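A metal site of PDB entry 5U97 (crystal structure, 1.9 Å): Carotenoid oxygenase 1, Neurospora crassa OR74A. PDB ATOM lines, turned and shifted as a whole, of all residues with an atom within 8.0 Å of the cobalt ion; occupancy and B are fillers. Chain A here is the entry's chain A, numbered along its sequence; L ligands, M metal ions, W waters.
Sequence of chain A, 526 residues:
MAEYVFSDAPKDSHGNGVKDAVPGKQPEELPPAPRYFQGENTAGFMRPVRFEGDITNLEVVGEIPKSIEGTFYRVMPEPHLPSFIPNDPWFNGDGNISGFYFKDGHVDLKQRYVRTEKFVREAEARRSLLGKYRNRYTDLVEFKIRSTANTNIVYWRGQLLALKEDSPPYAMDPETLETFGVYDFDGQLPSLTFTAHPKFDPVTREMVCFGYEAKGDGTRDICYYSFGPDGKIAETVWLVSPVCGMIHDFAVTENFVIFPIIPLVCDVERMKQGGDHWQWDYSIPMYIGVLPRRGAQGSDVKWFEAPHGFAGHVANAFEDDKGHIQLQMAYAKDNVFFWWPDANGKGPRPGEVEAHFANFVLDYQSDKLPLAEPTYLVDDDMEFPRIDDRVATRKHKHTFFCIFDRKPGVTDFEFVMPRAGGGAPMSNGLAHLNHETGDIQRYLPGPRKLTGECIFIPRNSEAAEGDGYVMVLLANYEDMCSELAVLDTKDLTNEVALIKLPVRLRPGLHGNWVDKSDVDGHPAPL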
ATOM      1  N   PHE A  91      -2.805  29.130  31.086  1.00  0.00           N
ATOM      2  CA  PHE A  91      -1.515  29.772  30.868  1.00  0.00           C
ATOM      3  C   PHE A  91      -0.864  30.258  32.157  1.00  0.00           C
ATOM      4  O   PHE A  91       0.288  30.678  32.127  1.00  0.00           O
ATOM      5  CB  PHE A  91      -1.613  30.981  29.919  1.00  0.00           C
ATOM      6  CG  PHE A  91      -2.096  30.734  28.522  1.00  0.00           C
ATOM      7  CD1 PHE A  91      -2.128  29.459  27.967  1.00  0.00           C
ATOM      8  CD2 PHE A  91      -2.564  31.795  27.748  1.00  0.00           C
ATOM      9  CE1 PHE A  91      -2.613  29.243  26.689  1.00  0.00           C
ATOM     10  CE2 PHE A  91      -3.071  31.581  26.468  1.00  0.00           C
ATOM     11  CZ  PHE A  91      -3.075  30.315  25.942  1.00  0.00           C
ATOM     12  N   THR A 151       5.976  27.898  28.989  1.00  0.00           N
ATOM     13  CA  THR A 151       5.476  28.009  27.628  1.00  0.00           C
ATOM     14  C   THR A 151       6.356  27.274  26.626  1.00  0.00           C
ATOM     15  O   THR A 151       5.831  26.622  25.737  1.00  0.00           O
ATOM     16  CB  THR A 151       5.263  29.477  27.235  1.00  0.00           C
ATOM     17  OG1 THR A 151       4.357  30.050  28.181  1.00  0.00           O
ATOM     18  CG2 THR A 151       4.714  29.631  25.830  1.00  0.00           C
ATOM     19  N   ASN A 152       7.681  27.416  26.740  1.00  0.00           N
ATOM     20  CA  ASN A 152       8.594  26.709  25.867  1.00  0.00           C
ATOM     21  C   ASN A 152       9.855  26.345  26.657  1.00  0.00           C
ATOM     22  O   ASN A 152      10.137  26.916  27.721  1.00  0.00           O
ATOM     23  CB  ASN A 152       8.921  27.514  24.601  1.00  0.00           C
ATOM     24  CG  ASN A 152       9.413  26.676  23.443  1.00  0.00           C
ATOM     25  OD1 ASN A 152       9.604  25.466  23.548  1.00  0.00           O
ATOM     26  ND2 ASN A 152       9.617  27.307  22.290  1.00  0.00           N
ATOM     27  N   GLU A 165       6.737  34.728  28.187  1.00  0.00           N
ATOM     28  CA  GLU A 165       6.897  35.955  27.411  1.00  0.00           C
ATOM     29  C   GLU A 165       6.802  37.237  28.258  1.00  0.00           C
ATOM     30  O   GLU A 165       7.027  38.312  27.712  1.00  0.00           O
ATOM     31  CB  GLU A 165       5.885  35.986  26.272  1.00  0.00           C
ATOM     32  CG  GLU A 165       4.431  36.068  26.691  1.00  0.00           C
ATOM     33  CD  GLU A 165       3.461  35.612  25.621  1.00  0.00           C
ATOM     34  OE1 GLU A 165       2.527  36.406  25.255  1.00  0.00           O
ATOM     35  OE2 GLU A 165       3.638  34.465  25.123  1.00  0.00           O
ATOM     36  N   THR A 195      10.772  36.335  24.496  1.00  0.00           N
ATOM     37  CA  THR A 195       9.712  35.594  23.822  1.00  0.00           C
ATOM     38  C   THR A 195       9.815  34.098  24.112  1.00  0.00           C
ATOM     39  O   THR A 195      10.906  33.572  24.306  1.00  0.00           O
ATOM     40  CB  THR A 195       9.791  35.823  22.302  1.00  0.00           C
ATOM     41  OG1 THR A 195       8.709  35.156  21.658  1.00  0.00           O
ATOM     42  CG2 THR A 195      11.088  35.331  21.698  1.00  0.00           C
ATOM     43  N   ALA A 196       8.669  33.415  24.040  1.00  0.00           N
ATOM     44  CA  ALA A 196       8.646  31.973  24.099  1.00  0.00           C
ATOM     45  C   ALA A 196       9.035  31.356  22.756  1.00  0.00           C
ATOM     46  O   ALA A 196       9.152  30.135  22.672  1.00  0.00           O
ATOM     47  CB  ALA A 196       7.283  31.504  24.539  1.00  0.00           C
ATOM     48  N   HIS A 197       9.246  32.160  21.704  1.00  0.00           N
ATOM     49  CA  HIS A 197       9.467  31.628  20.367  1.00  0.00           C
ATOM     50  C   HIS A 197      10.693  32.249  19.699  1.00  0.00           C
ATOM     51  O   HIS A 197      10.601  32.769  18.596  1.00  0.00           O
ATOM     52  CB  HIS A 197       8.199  31.783  19.527  1.00  0.00           C
ATOM     53  CG  HIS A 197       7.126  30.861  19.966  1.00  0.00           C
ATOM     54  ND1 HIS A 197       7.231  29.507  19.743  1.00  0.00           N
ATOM     55  CD2 HIS A 197       5.952  31.049  20.604  1.00  0.00           C
ATOM     56  CE1 HIS A 197       6.163  28.901  20.236  1.00  0.00           C
ATOM     57  NE2 HIS A 197       5.364  29.825  20.766  1.00  0.00           N
ATOM     58  N   HIS A 248       2.806  36.935  20.514  1.00  0.00           N
ATOM     59  CA  HIS A 248       3.157  35.627  21.061  1.00  0.00           C
ATOM     60  C   HIS A 248       4.301  34.973  20.284  1.00  0.00           C
ATOM     61  O   HIS A 248       5.192  34.342  20.869  1.00  0.00           O
ATOM     62  CB  HIS A 248       1.941  34.701  21.108  1.00  0.00           C
ATOM     63  CG  HIS A 248       2.314  33.355  21.641  1.00  0.00           C
ATOM     64  ND1 HIS A 248       2.720  33.194  22.943  1.00  0.00           N
ATOM     65  CD2 HIS A 248       2.420  32.152  21.049  1.00  0.00           C
ATOM     66  CE1 HIS A 248       3.042  31.916  23.144  1.00  0.00           C
ATOM     67  NE2 HIS A 248       2.864  31.269  22.008  1.00  0.00           N
ATOM     68  N   ASP A 249       4.259  35.092  18.951  1.00  0.00           N
ATOM     69  CA  ASP A 249       5.226  34.450  18.079  1.00  0.00           C
ATOM     70  C   ASP A 249       5.754  35.500  17.114  1.00  0.00           C
ATOM     71  O   ASP A 249       5.198  36.590  17.033  1.00  0.00           O
ATOM     72  CB  ASP A 249       4.574  33.236  17.398  1.00  0.00           C
ATOM     73  CG  ASP A 249       5.537  32.194  16.837  1.00  0.00           C
ATOM     74  OD1 ASP A 249       6.763  32.467  16.815  1.00  0.00           O
ATOM     75  OD2 ASP A 249       5.039  31.124  16.436  1.00  0.00           O
ATOM     76  N   GLY A 312      -1.974  33.276  15.068  1.00  0.00           N
ATOM     77  CA  GLY A 312      -1.549  31.996  15.626  1.00  0.00           C
ATOM     78  C   GLY A 312      -0.055  31.735  15.375  1.00  0.00           C
ATOM     79  O   GLY A 312       0.672  32.615  14.956  1.00  0.00           O
ATOM     80  N   HIS A 313       0.392  30.506  15.636  1.00  0.00           N
ATOM     81  CA  HIS A 313       1.798  30.161  15.585  1.00  0.00           C
ATOM     82  C   HIS A 313       2.335  30.222  14.162  1.00  0.00           C
ATOM     83  O   HIS A 313       1.646  29.859  13.199  1.00  0.00           O
ATOM     84  CB  HIS A 313       2.050  28.772  16.187  1.00  0.00           C
ATOM     85  CG  HIS A 313       2.005  28.760  17.669  1.00  0.00           C
ATOM     86  ND1 HIS A 313       0.979  28.197  18.400  1.00  0.00           N
ATOM     87  CD2 HIS A 313       2.852  29.270  18.553  1.00  0.00           C
ATOM     88  CE1 HIS A 313       1.244  28.351  19.691  1.00  0.00           C
ATOM     89  NE2 HIS A 313       2.365  29.003  19.803  1.00  0.00           N
ATOM     90  N   VAL A 314       3.590  30.647  14.051  1.00  0.00           N
ATOM     91  CA  VAL A 314       4.297  30.731  12.789  1.00  0.00           C
ATOM     92  C   VAL A 314       4.912  29.364  12.474  1.00  0.00           C
ATOM     93  O   VAL A 314       5.656  28.809  13.274  1.00  0.00           O
ATOM     94  CB  VAL A 314       5.393  31.808  12.867  1.00  0.00           C
ATOM     95  CG1 VAL A 314       6.285  31.823  11.634  1.00  0.00           C
ATOM     96  CG2 VAL A 314       4.781  33.180  13.125  1.00  0.00           C
ATOM     97  N   PHE A 337      -8.536  33.220  22.217  1.00  0.00           N
ATOM     98  CA  PHE A 337      -8.500  33.322  23.667  1.00  0.00           C
ATOM     99  C   PHE A 337      -9.791  33.990  24.155  1.00  0.00           C
ATOM    100  O   PHE A 337      -9.792  35.107  24.670  1.00  0.00           O
ATOM    101  CB  PHE A 337      -7.232  34.058  24.116  1.00  0.00           C
ATOM    102  CG  PHE A 337      -5.919  33.447  23.693  1.00  0.00           C
ATOM    103  CD1 PHE A 337      -5.841  32.160  23.187  1.00  0.00           C
ATOM    104  CD2 PHE A 337      -4.750  34.186  23.761  1.00  0.00           C
ATOM    105  CE1 PHE A 337      -4.626  31.626  22.788  1.00  0.00           C
ATOM    106  CE2 PHE A 337      -3.534  33.652  23.362  1.00  0.00           C
ATOM    107  CZ  PHE A 337      -3.469  32.364  22.883  1.00  0.00           C
ATOM    108  N   GLU A 383      -3.227  23.994  14.155  1.00  0.00           N
ATOM    109  CA  GLU A 383      -2.341  24.829  14.958  1.00  0.00           C
ATOM    110  C   GLU A 383      -1.046  24.061  15.245  1.00  0.00           C
ATOM    111  O   GLU A 383      -0.875  22.922  14.799  1.00  0.00           O
ATOM    112  CB  GLU A 383      -3.034  25.311  16.239  1.00  0.00           C
ATOM    113  CG  GLU A 383      -3.307  26.818  16.280  1.00  0.00           C
ATOM    114  CD  GLU A 383      -2.110  27.724  16.555  1.00  0.00           C
ATOM    115  OE1 GLU A 383      -0.965  27.228  16.663  1.00  0.00           O
ATOM    116  OE2 GLU A 383      -2.329  28.959  16.657  1.00  0.00           O
ATOM    117  N   PHE A 384      -0.123  24.730  15.956  1.00  0.00           N
ATOM    118  CA  PHE A 384       1.115  24.131  16.447  1.00  0.00           C
ATOM    119  C   PHE A 384       1.932  23.554  15.298  1.00  0.00           C
ATOM    120  O   PHE A 384       2.326  22.389  15.329  1.00  0.00           O
ATOM    121  CB  PHE A 384       0.795  23.096  17.520  1.00  0.00           C
ATOM    122  CG  PHE A 384      -0.192  23.587  18.549  1.00  0.00           C
ATOM    123  CD1 PHE A 384      -1.423  22.971  18.689  1.00  0.00           C
ATOM    124  CD2 PHE A 384       0.095  24.699  19.332  1.00  0.00           C
ATOM    125  CE1 PHE A 384      -2.342  23.443  19.615  1.00  0.00           C
ATOM    126  CE2 PHE A 384      -0.827  25.166  20.246  1.00  0.00           C
ATOM    127  CZ  PHE A 384      -2.036  24.540  20.385  1.00  0.00           C
ATOM    128  N   GLU A 453       1.562  19.032  20.797  1.00  0.00           N
ATOM    129  CA  GLU A 453       2.421  19.489  19.727  1.00  0.00           C
ATOM    130  C   GLU A 453       3.466  18.410  19.432  1.00  0.00           C
ATOM    131  O   GLU A 453       4.056  17.844  20.350  1.00  0.00           O
ATOM    132  CB  GLU A 453       3.110  20.798  20.138  1.00  0.00           C
ATOM    133  CG  GLU A 453       4.111  21.338  19.126  1.00  0.00           C
ATOM    134  CD  GLU A 453       5.015  22.427  19.672  1.00  0.00           C
ATOM    135  OE1 GLU A 453       5.829  22.130  20.581  1.00  0.00           O
ATOM    136  OE2 GLU A 453       4.920  23.585  19.185  1.00  0.00           O
ATOM    137  N   LEU A 509       2.309  22.841  26.553  1.00  0.00           N
ATOM    138  CA  LEU A 509       2.572  23.801  25.499  1.00  0.00           C
ATOM    139  C   LEU A 509       3.698  23.253  24.639  1.00  0.00           C
ATOM    140  O   LEU A 509       3.544  22.147  24.101  1.00  0.00           O
ATOM    141  CB  LEU A 509       2.806  25.176  26.147  1.00  0.00           C
ATOM    142  CG  LEU A 509       1.545  25.822  26.730  1.00  0.00           C
ATOM    143  CD1 LEU A 509       1.873  27.029  27.591  1.00  0.00           C
ATOM    144  CD2 LEU A 509       0.588  26.211  25.625  1.00  0.00           C
ATOM    145  N   HIS A 510       4.828  23.946  24.547  1.00  0.00           N
ATOM    146  CA  HIS A 510       5.803  23.652  23.499  1.00  0.00           C
ATOM    147  C   HIS A 510       6.848  22.653  23.973  1.00  0.00           C
ATOM    148  O   HIS A 510       7.043  22.441  25.173  1.00  0.00           O
ATOM    149  CB  HIS A 510       6.410  24.954  22.962  1.00  0.00           C
ATOM    150  CG  HIS A 510       5.395  25.834  22.317  1.00  0.00           C
ATOM    151  ND1 HIS A 510       4.823  25.535  21.100  1.00  0.00           N
ATOM    152  CD2 HIS A 510       4.849  27.008  22.714  1.00  0.00           C
ATOM    153  CE1 HIS A 510       3.947  26.490  20.790  1.00  0.00           C
ATOM    154  NE2 HIS A 510       3.954  27.398  21.749  1.00  0.00           N
HETATM  155  C1  LIG L   1      -1.688  29.845  19.959  1.00  0.00           C
HETATM  156  C2  LIG L   1      -2.530  28.745  20.024  1.00  0.00           C
HETATM  157  C3  LIG L   1      -2.703  28.095  21.240  1.00  0.00           C
HETATM  158  C4  LIG L   1      -2.028  28.534  22.370  1.00  0.00           C
HETATM  159  C5  LIG L   1      -1.205  29.651  22.319  1.00  0.00           C
HETATM  160  C6  LIG L   1      -1.035  30.313  21.099  1.00  0.00           C
HETATM  161  C7  LIG L   1      -0.560  30.050  23.581  1.00  0.00           C
HETATM  162  C8  LIG L   1      -0.099  31.242  23.912  1.00  0.00           C
HETATM  163  C9  LIG L   1       0.390  31.661  25.226  1.00  0.00           C
HETATM  164  C10 LIG L   1       0.752  30.767  26.255  1.00  0.00           C
HETATM  165  C11 LIG L   1       1.182  31.232  27.495  1.00  0.00           C
HETATM  166  C12 LIG L   1       1.206  32.608  27.741  1.00  0.00           C
HETATM  167  C13 LIG L   1       0.825  33.495  26.750  1.00  0.00           C
HETATM  168  C14 LIG L   1       0.410  33.014  25.521  1.00  0.00           C
HETATM  169  O1  LIG L   1       1.606  33.137  28.941  1.00  0.00           O
HETATM  170  O2  LIG L   1      -3.515  27.017  21.421  1.00  0.00           O
HETATM  171  O3  LIG L   1      -1.524  30.530  18.763  1.00  0.00           O
HETATM  172  O4  LIG L   1       1.579  30.374  28.517  1.00  0.00           O
HETATM  173 CO    CO M   1       3.457  29.396  21.451  1.00  0.00          CO
HETATM  174  O   HOH W   1       1.968  28.768  23.356  1.00  0.00           O
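A ring nitrogen (ND1) of His 313 lies within hydrogen-bond range of an oxygen (O3) of the ligand, at 3.4 Å. An oxygen (O3) of the ligand sits at hydrogen-bond distance from the side-chain carboxylate (OE2) of Glu 383. OG1 of Thr 151 sits at hydrogen-bond distance from O4 of the ligand (2.8 Å).
The backbone NH of His 197 lies within hydrogen-bond range of the side-chain hydroxyl of Thr 195, at 3.0 Å. ND1 of His 248 is in hydrogen-bond range of OE2 of Glu 165, 2.7 Å away. N of His 510 is in hydrogen-bond range of O of Thr 151, at 3.1 Å. ND1 of His 510 is in hydrogen-bond range of OE2 of Glu 453 (2.7 Å). ND1 of His 313 sits at hydrogen-bond distance from OE1 of Glu 383, 2.8 Å away.
Of the 18 residues printed, 4 come within 4 Å of the cobalt ion.
The cobalt ion is bound by a ring nitrogen (NE2) of His 313 (2.0 Å), a ring nitrogen (NE2) of His 248 (2.0 Å), a ring nitrogen (NE2) of His 197 (2.1 Å), a ring nitrogen (NE2) of His 510 (2.1 Å) and water W1 (2.5 Å). The cobalt ion has five donor atoms within binding distance.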
